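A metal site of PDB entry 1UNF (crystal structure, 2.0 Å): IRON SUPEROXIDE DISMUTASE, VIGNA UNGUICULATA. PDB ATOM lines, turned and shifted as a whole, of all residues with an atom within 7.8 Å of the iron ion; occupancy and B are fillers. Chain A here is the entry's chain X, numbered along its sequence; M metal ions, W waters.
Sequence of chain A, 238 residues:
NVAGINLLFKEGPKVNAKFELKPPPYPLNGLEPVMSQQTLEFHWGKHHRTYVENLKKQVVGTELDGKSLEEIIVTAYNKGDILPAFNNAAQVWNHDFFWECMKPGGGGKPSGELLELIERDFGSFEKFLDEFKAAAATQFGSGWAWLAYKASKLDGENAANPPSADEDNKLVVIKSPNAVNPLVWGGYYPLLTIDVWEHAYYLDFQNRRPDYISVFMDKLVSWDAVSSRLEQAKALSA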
ATOM      1  N   HIS A  43       9.423  -7.632  23.495  1.00  0.00           N
ATOM      2  CA  HIS A  43      10.696  -6.984  23.804  1.00  0.00           C
ATOM      3  C   HIS A  43      11.487  -6.759  22.507  1.00  0.00           C
ATOM      4  O   HIS A  43      11.945  -5.651  22.233  1.00  0.00           O
ATOM      5  CB  HIS A  43      11.458  -7.830  24.843  1.00  0.00           C
ATOM      6  CG  HIS A  43      12.609  -7.124  25.476  1.00  0.00           C
ATOM      7  ND1 HIS A  43      13.403  -7.712  26.443  1.00  0.00           N
ATOM      8  CD2 HIS A  43      13.095  -5.868  25.313  1.00  0.00           C
ATOM      9  CE1 HIS A  43      14.337  -6.857  26.829  1.00  0.00           C
ATOM     10  NE2 HIS A  43      14.171  -5.734  26.157  1.00  0.00           N
ATOM     11  N   TRP A  44      11.630  -7.808  21.732  1.00  0.00           N
ATOM     12  CA  TRP A  44      12.214  -7.714  20.396  1.00  0.00           C
ATOM     13  C   TRP A  44      11.265  -7.114  19.324  1.00  0.00           C
ATOM     14  O   TRP A  44      11.612  -6.174  18.615  1.00  0.00           O
ATOM     15  CB  TRP A  44      12.647  -9.124  19.909  1.00  0.00           C
ATOM     16  CG  TRP A  44      13.243  -9.114  18.521  1.00  0.00           C
ATOM     17  CD1 TRP A  44      14.517  -8.717  18.185  1.00  0.00           C
ATOM     18  CD2 TRP A  44      12.602  -9.494  17.293  1.00  0.00           C
ATOM     19  NE1 TRP A  44      14.703  -8.826  16.834  1.00  0.00           N
ATOM     20  CE2 TRP A  44      13.552  -9.323  16.261  1.00  0.00           C
ATOM     21  CE3 TRP A  44      11.324  -9.984  16.976  1.00  0.00           C
ATOM     22  CZ2 TRP A  44      13.258  -9.606  14.917  1.00  0.00           C
ATOM     23  CZ3 TRP A  44      11.021 -10.284  15.621  1.00  0.00           C
ATOM     24  CH2 TRP A  44      11.989 -10.080  14.611  1.00  0.00           C
ATOM     25  N   HIS A  47       9.514  -3.264  21.294  1.00  0.00           N
ATOM     26  CA  HIS A  47      10.466  -2.304  21.853  1.00  0.00           C
ATOM     27  C   HIS A  47      11.721  -2.141  20.971  1.00  0.00           C
ATOM     28  O   HIS A  47      12.086  -1.040  20.522  1.00  0.00           O
ATOM     29  CB  HIS A  47      10.883  -2.781  23.263  1.00  0.00           C
ATOM     30  CG  HIS A  47       9.789  -2.745  24.280  1.00  0.00           C
ATOM     31  ND1 HIS A  47       9.555  -1.656  25.083  1.00  0.00           N
ATOM     32  CD2 HIS A  47       8.865  -3.678  24.627  1.00  0.00           C
ATOM     33  CE1 HIS A  47       8.524  -1.919  25.889  1.00  0.00           C
ATOM     34  NE2 HIS A  47       8.090  -3.138  25.627  1.00  0.00           N
ATOM     35  N   HIS A  48      12.368  -3.263  20.700  1.00  0.00           N
ATOM     36  CA  HIS A  48      13.606  -3.269  19.931  1.00  0.00           C
ATOM     37  C   HIS A  48      13.310  -2.754  18.522  1.00  0.00           C
ATOM     38  O   HIS A  48      13.995  -1.860  18.021  1.00  0.00           O
ATOM     39  CB  HIS A  48      14.155  -4.687  19.904  1.00  0.00           C
ATOM     40  CG  HIS A  48      15.572  -4.799  19.433  1.00  0.00           C
ATOM     41  ND1 HIS A  48      16.283  -5.984  19.499  1.00  0.00           N
ATOM     42  CD2 HIS A  48      16.416  -3.891  18.866  1.00  0.00           C
ATOM     43  CE1 HIS A  48      17.486  -5.806  18.983  1.00  0.00           C
ATOM     44  NE2 HIS A  48      17.598  -4.550  18.595  1.00  0.00           N
ATOM     45  N   TYR A  51      12.921   1.117  18.569  1.00  0.00           N
ATOM     46  CA  TYR A  51      14.226   1.755  18.592  1.00  0.00           C
ATOM     47  C   TYR A  51      14.852   1.796  17.187  1.00  0.00           C
ATOM     48  O   TYR A  51      15.448   2.804  16.820  1.00  0.00           O
ATOM     49  CB  TYR A  51      15.172   1.027  19.548  1.00  0.00           C
ATOM     50  CG  TYR A  51      14.799   1.152  21.025  1.00  0.00           C
ATOM     51  CD1 TYR A  51      14.590   2.407  21.607  1.00  0.00           C
ATOM     52  CD2 TYR A  51      14.658   0.020  21.819  1.00  0.00           C
ATOM     53  CE1 TYR A  51      14.236   2.520  22.971  1.00  0.00           C
ATOM     54  CE2 TYR A  51      14.305   0.115  23.200  1.00  0.00           C
ATOM     55  CZ  TYR A  51      14.094   1.348  23.752  1.00  0.00           C
ATOM     56  OH  TYR A  51      13.789   1.408  25.085  1.00  0.00           O
ATOM     57  N   GLN A  91      20.104   1.863  22.424  1.00  0.00           N
ATOM     58  CA  GLN A  91      19.174   0.799  22.767  1.00  0.00           C
ATOM     59  C   GLN A  91      19.152  -0.262  21.662  1.00  0.00           C
ATOM     60  O   GLN A  91      18.975  -1.443  21.958  1.00  0.00           O
ATOM     61  CB  GLN A  91      17.751   1.351  23.035  1.00  0.00           C
ATOM     62  CG  GLN A  91      17.598   2.105  24.386  1.00  0.00           C
ATOM     63  CD  GLN A  91      17.613   1.145  25.578  1.00  0.00           C
ATOM     64  OE1 GLN A  91      18.667   0.700  25.984  1.00  0.00           O
ATOM     65  NE2 GLN A  91      16.431   0.820  26.117  1.00  0.00           N
ATOM     66  N   ASN A  94      22.376  -2.199  22.496  1.00  0.00           N
ATOM     67  CA  ASN A  94      22.159  -2.929  23.763  1.00  0.00           C
ATOM     68  C   ASN A  94      21.275  -4.171  23.597  1.00  0.00           C
ATOM     69  O   ASN A  94      21.558  -5.240  24.116  1.00  0.00           O
ATOM     70  CB  ASN A  94      21.516  -1.997  24.815  1.00  0.00           C
ATOM     71  CG  ASN A  94      22.376  -0.833  25.169  1.00  0.00           C
ATOM     72  OD1 ASN A  94      23.585  -0.881  24.971  1.00  0.00           O
ATOM     73  ND2 ASN A  94      21.765   0.253  25.702  1.00  0.00           N
ATOM     74  N   HIS A  95      20.176  -4.028  22.876  1.00  0.00           N
ATOM     75  CA  HIS A  95      19.300  -5.170  22.644  1.00  0.00           C
ATOM     76  C   HIS A  95      19.881  -6.182  21.674  1.00  0.00           C
ATOM     77  O   HIS A  95      19.743  -7.373  21.899  1.00  0.00           O
ATOM     78  CB  HIS A  95      17.955  -4.701  22.157  1.00  0.00           C
ATOM     79  CG  HIS A  95      17.134  -4.033  23.229  1.00  0.00           C
ATOM     80  ND1 HIS A  95      17.263  -2.689  23.535  1.00  0.00           N
ATOM     81  CD2 HIS A  95      16.226  -4.544  24.085  1.00  0.00           C
ATOM     82  CE1 HIS A  95      16.445  -2.397  24.522  1.00  0.00           C
ATOM     83  NE2 HIS A  95      15.804  -3.499  24.881  1.00  0.00           N
ATOM     84  N   PHE A  98      22.128  -7.959  23.929  1.00  0.00           N
ATOM     85  CA  PHE A  98      21.320  -8.718  24.892  1.00  0.00           C
ATOM     86  C   PHE A  98      20.846 -10.070  24.331  1.00  0.00           C
ATOM     87  O   PHE A  98      21.022 -11.103  24.984  1.00  0.00           O
ATOM     88  CB  PHE A  98      20.157  -7.856  25.390  1.00  0.00           C
ATOM     89  CG  PHE A  98      19.268  -8.552  26.424  1.00  0.00           C
ATOM     90  CD1 PHE A  98      19.795  -8.989  27.648  1.00  0.00           C
ATOM     91  CD2 PHE A  98      17.904  -8.714  26.188  1.00  0.00           C
ATOM     92  CE1 PHE A  98      18.954  -9.606  28.594  1.00  0.00           C
ATOM     93  CE2 PHE A  98      17.064  -9.331  27.135  1.00  0.00           C
ATOM     94  CZ  PHE A  98      17.586  -9.773  28.335  1.00  0.00           C
ATOM     95  N   TRP A  99      20.281 -10.080  23.112  1.00  0.00           N
ATOM     96  CA  TRP A  99      19.864 -11.337  22.497  1.00  0.00           C
ATOM     97  C   TRP A  99      21.056 -12.320  22.301  1.00  0.00           C
ATOM     98  O   TRP A  99      20.905 -13.526  22.524  1.00  0.00           O
ATOM     99  CB  TRP A  99      19.154 -11.122  21.156  1.00  0.00           C
ATOM    100  CG  TRP A  99      17.991 -10.166  21.271  1.00  0.00           C
ATOM    101  CD1 TRP A  99      17.771  -9.061  20.512  1.00  0.00           C
ATOM    102  CD2 TRP A  99      16.946 -10.210  22.240  1.00  0.00           C
ATOM    103  NE1 TRP A  99      16.628  -8.433  20.909  1.00  0.00           N
ATOM    104  CE2 TRP A  99      16.120  -9.107  21.985  1.00  0.00           C
ATOM    105  CE3 TRP A  99      16.630 -11.083  23.273  1.00  0.00           C
ATOM    106  CZ2 TRP A  99      14.972  -8.853  22.744  1.00  0.00           C
ATOM    107  CZ3 TRP A  99      15.507 -10.849  24.013  1.00  0.00           C
ATOM    108  CH2 TRP A  99      14.682  -9.732  23.756  1.00  0.00           C
ATOM    109  N   GLY A 143      17.620   0.313  33.135  1.00  0.00           N
ATOM    110  CA  GLY A 143      19.034   0.276  32.802  1.00  0.00           C
ATOM    111  C   GLY A 143      19.544  -1.130  32.596  1.00  0.00           C
ATOM    112  O   GLY A 143      18.780  -2.026  32.252  1.00  0.00           O
ATOM    113  N   TRP A 144      20.844  -1.304  32.809  1.00  0.00           N
ATOM    114  CA  TRP A 144      21.562  -2.506  32.364  1.00  0.00           C
ATOM    115  C   TRP A 144      22.570  -2.866  33.414  1.00  0.00           C
ATOM    116  O   TRP A 144      23.045  -1.986  34.139  1.00  0.00           O
ATOM    117  CB  TRP A 144      22.289  -2.278  31.003  1.00  0.00           C
ATOM    118  CG  TRP A 144      21.311  -1.912  29.920  1.00  0.00           C
ATOM    119  CD1 TRP A 144      20.825  -0.654  29.645  1.00  0.00           C
ATOM    120  CD2 TRP A 144      20.767  -2.779  28.925  1.00  0.00           C
ATOM    121  NE1 TRP A 144      19.953  -0.719  28.572  1.00  0.00           N
ATOM    122  CE2 TRP A 144      19.889  -2.018  28.126  1.00  0.00           C
ATOM    123  CE3 TRP A 144      20.893  -4.164  28.677  1.00  0.00           C
ATOM    124  CZ2 TRP A 144      19.154  -2.572  27.068  1.00  0.00           C
ATOM    125  CZ3 TRP A 144      20.177  -4.710  27.625  1.00  0.00           C
ATOM    126  CH2 TRP A 144      19.304  -3.912  26.830  1.00  0.00           C
ATOM    127  N   ASN A 178      19.278   3.518  32.009  1.00  0.00           N
ATOM    128  CA  ASN A 178      18.589   3.874  30.778  1.00  0.00           C
ATOM    129  C   ASN A 178      19.245   3.193  29.557  1.00  0.00           C
ATOM    130  O   ASN A 178      19.228   1.954  29.476  1.00  0.00           O
ATOM    131  CB  ASN A 178      18.486   5.422  30.670  1.00  0.00           C
ATOM    132  CG  ASN A 178      17.531   6.039  31.716  1.00  0.00           C
ATOM    133  OD1 ASN A 178      17.583   7.255  31.986  1.00  0.00           O
ATOM    134  ND2 ASN A 178      16.700   5.211  32.315  1.00  0.00           N
ATOM    135  N   ASP A 195      19.396  -6.892  30.644  1.00  0.00           N
ATOM    136  CA  ASP A 195      18.482  -5.747  30.553  1.00  0.00           C
ATOM    137  C   ASP A 195      17.669  -5.740  31.816  1.00  0.00           C
ATOM    138  O   ASP A 195      16.998  -6.748  32.105  1.00  0.00           O
ATOM    139  CB  ASP A 195      17.528  -5.991  29.353  1.00  0.00           C
ATOM    140  CG  ASP A 195      16.639  -4.773  29.018  1.00  0.00           C
ATOM    141  OD1 ASP A 195      16.617  -3.783  29.807  1.00  0.00           O
ATOM    142  OD2 ASP A 195      15.965  -4.809  27.982  1.00  0.00           O
ATOM    143  N   VAL A 196      17.705  -4.649  32.583  1.00  0.00           N
ATOM    144  CA  VAL A 196      16.829  -4.545  33.782  1.00  0.00           C
ATOM    145  C   VAL A 196      15.703  -3.496  33.710  1.00  0.00           C
ATOM    146  O   VAL A 196      15.048  -3.167  34.728  1.00  0.00           O
ATOM    147  CB  VAL A 196      17.601  -4.529  35.127  1.00  0.00           C
ATOM    148  CG1 VAL A 196      18.367  -5.846  35.262  1.00  0.00           C
ATOM    149  CG2 VAL A 196      18.556  -3.270  35.286  1.00  0.00           C
ATOM    150  N   TRP A 197      15.489  -2.953  32.499  1.00  0.00           N
ATOM    151  CA  TRP A 197      14.217  -2.335  32.199  1.00  0.00           C
ATOM    152  C   TRP A 197      13.105  -3.287  32.556  1.00  0.00           C
ATOM    153  O   TRP A 197      13.203  -4.492  32.295  1.00  0.00           O
ATOM    154  CB  TRP A 197      14.103  -1.979  30.731  1.00  0.00           C
ATOM    155  CG  TRP A 197      14.947  -0.868  30.259  1.00  0.00           C
ATOM    156  CD1 TRP A 197      16.313  -0.761  30.319  1.00  0.00           C
ATOM    157  CD2 TRP A 197      14.476   0.347  29.675  1.00  0.00           C
ATOM    158  NE1 TRP A 197      16.711   0.448  29.779  1.00  0.00           N
ATOM    159  CE2 TRP A 197      15.611   1.133  29.359  1.00  0.00           C
ATOM    160  CE3 TRP A 197      13.201   0.831  29.363  1.00  0.00           C
ATOM    161  CZ2 TRP A 197      15.512   2.387  28.765  1.00  0.00           C
ATOM    162  CZ3 TRP A 197      13.101   2.064  28.739  1.00  0.00           C
ATOM    163  CH2 TRP A 197      14.239   2.839  28.472  1.00  0.00           C
ATOM    164  N   GLU A 198      12.019  -2.754  33.115  1.00  0.00           N
ATOM    165  CA  GLU A 198      10.921  -3.606  33.532  1.00  0.00           C
ATOM    166  C   GLU A 198      10.305  -4.406  32.375  1.00  0.00           C
ATOM    167  O   GLU A 198       9.854  -5.519  32.564  1.00  0.00           O
ATOM    168  CB  GLU A 198       9.859  -2.800  34.303  1.00  0.00           C
ATOM    169  CG  GLU A 198      10.352  -2.449  35.697  1.00  0.00           C
ATOM    170  CD  GLU A 198       9.430  -1.526  36.468  1.00  0.00           C
ATOM    171  OE1 GLU A 198       8.833  -0.642  35.843  1.00  0.00           O
ATOM    172  OE2 GLU A 198       9.328  -1.687  37.733  1.00  0.00           O
ATOM    173  N   HIS A 199      10.286  -3.843  31.191  1.00  0.00           N
ATOM    174  CA  HIS A 199       9.754  -4.631  30.069  1.00  0.00           C
ATOM    175  C   HIS A 199      10.498  -5.951  29.778  1.00  0.00           C
ATOM    176  O   HIS A 199       9.924  -6.871  29.177  1.00  0.00           O
ATOM    177  CB  HIS A 199       9.659  -3.777  28.811  1.00  0.00           C
ATOM    178  CG  HIS A 199      10.975  -3.393  28.238  1.00  0.00           C
ATOM    179  ND1 HIS A 199      11.320  -2.078  28.019  1.00  0.00           N
ATOM    180  CD2 HIS A 199      12.011  -4.142  27.768  1.00  0.00           C
ATOM    181  CE1 HIS A 199      12.531  -2.029  27.483  1.00  0.00           C
ATOM    182  NE2 HIS A 199      12.958  -3.263  27.287  1.00  0.00           N
ATOM    183  N   ALA A 200      11.776  -6.025  30.169  1.00  0.00           N
ATOM    184  CA  ALA A 200      12.552  -7.250  29.948  1.00  0.00           C
ATOM    185  C   ALA A 200      12.000  -8.417  30.768  1.00  0.00           C
ATOM    186  O   ALA A 200      12.221  -9.555  30.410  1.00  0.00           O
ATOM    187  CB  ALA A 200      14.042  -7.038  30.330  1.00  0.00           C
ATOM    188  N   TYR A 201      11.336  -8.124  31.881  1.00  0.00           N
ATOM    189  CA  TYR A 201      10.942  -9.180  32.800  1.00  0.00           C
ATOM    190  C   TYR A 201       9.521  -9.125  33.306  1.00  0.00           C
ATOM    191  O   TYR A 201       9.047 -10.102  33.956  1.00  0.00           O
ATOM    192  CB  TYR A 201      11.905  -9.260  33.985  1.00  0.00           C
ATOM    193  CG  TYR A 201      12.033  -8.025  34.858  1.00  0.00           C
ATOM    194  CD1 TYR A 201      11.157  -7.789  35.935  1.00  0.00           C
ATOM    195  CD2 TYR A 201      13.031  -7.092  34.590  1.00  0.00           C
ATOM    196  CE1 TYR A 201      11.299  -6.638  36.734  1.00  0.00           C
ATOM    197  CE2 TYR A 201      13.172  -5.961  35.360  1.00  0.00           C
ATOM    198  CZ  TYR A 201      12.310  -5.743  36.458  1.00  0.00           C
ATOM    199  OH  TYR A 201      12.523  -4.613  37.238  1.00  0.00           O
ATOM    200  N   TYR A 212      14.188 -12.897  38.320  1.00  0.00           N
ATOM    201  CA  TYR A 212      14.571 -12.768  36.908  1.00  0.00           C
ATOM    202  C   TYR A 212      16.089 -12.819  36.658  1.00  0.00           C
ATOM    203  O   TYR A 212      16.547 -13.523  35.770  1.00  0.00           O
ATOM    204  CB  TYR A 212      14.005 -11.459  36.370  1.00  0.00           C
ATOM    205  CG  TYR A 212      14.655 -10.939  35.092  1.00  0.00           C
ATOM    206  CD1 TYR A 212      14.573 -11.665  33.887  1.00  0.00           C
ATOM    207  CD2 TYR A 212      15.285  -9.720  35.082  1.00  0.00           C
ATOM    208  CE1 TYR A 212      15.129 -11.188  32.725  1.00  0.00           C
ATOM    209  CE2 TYR A 212      15.864  -9.219  33.900  1.00  0.00           C
ATOM    210  CZ  TYR A 212      15.769  -9.937  32.722  1.00  0.00           C
ATOM    211  OH  TYR A 212      16.343  -9.409  31.565  1.00  0.00           O
HETATM  212 FE    FE M   1      14.932  -3.806  26.782  1.00  0.00          FE
HETATM  213  O   HOH W   1      15.759  -1.959  27.512  1.00  0.00           O
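The side-chain carboxylate (OD2) of Asp 195 binds the iron ion, at 1.9 Å. A ring nitrogen (NE2) of His 199 is bound to the iron ion (2.1 Å). A ring nitrogen (NE2) of His 95 is bound to the iron ion, at 2.1 Å. The iron ion is bound by water W1 (2.2 Å). NE2 of His 43 is bound to the iron ion. The iron ion has five donor atoms within binding distance.
The side-chain carboxylate of Asp 195 lies within hydrogen-bond range of the backbone NH of Trp 197 (3.0 Å). The backbone carbonyl oxygen of Asp 195 is in hydrogen-bond range of the side-chain hydroxyl of Tyr 212 (2.8 Å). A ring nitrogen (ND1) of His 199 sits at hydrogen-bond distance from a ring nitrogen (ND1) of His 47. ND1 of His 95 is in hydrogen-bond range of O of Gln 91, 2.6 Å away. O of His 95 sits close to NE1 of Trp 99, at 3.4 Å. O of His 43 sits at hydrogen-bond distance from N of His 48, at 2.9 Å.
Water W1 lies within hydrogen-bond range of the side-chain carboxylate of Asp 195 (3.1 Å), the side-chain amide nitrogen of Gln 91 (3.2 Å) and the indole nitrogen of Trp 197 (3.4 Å).
Four residues have an atom within 4 Å of the iron ion: His 43, His 95, Asp 195 and His 199.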
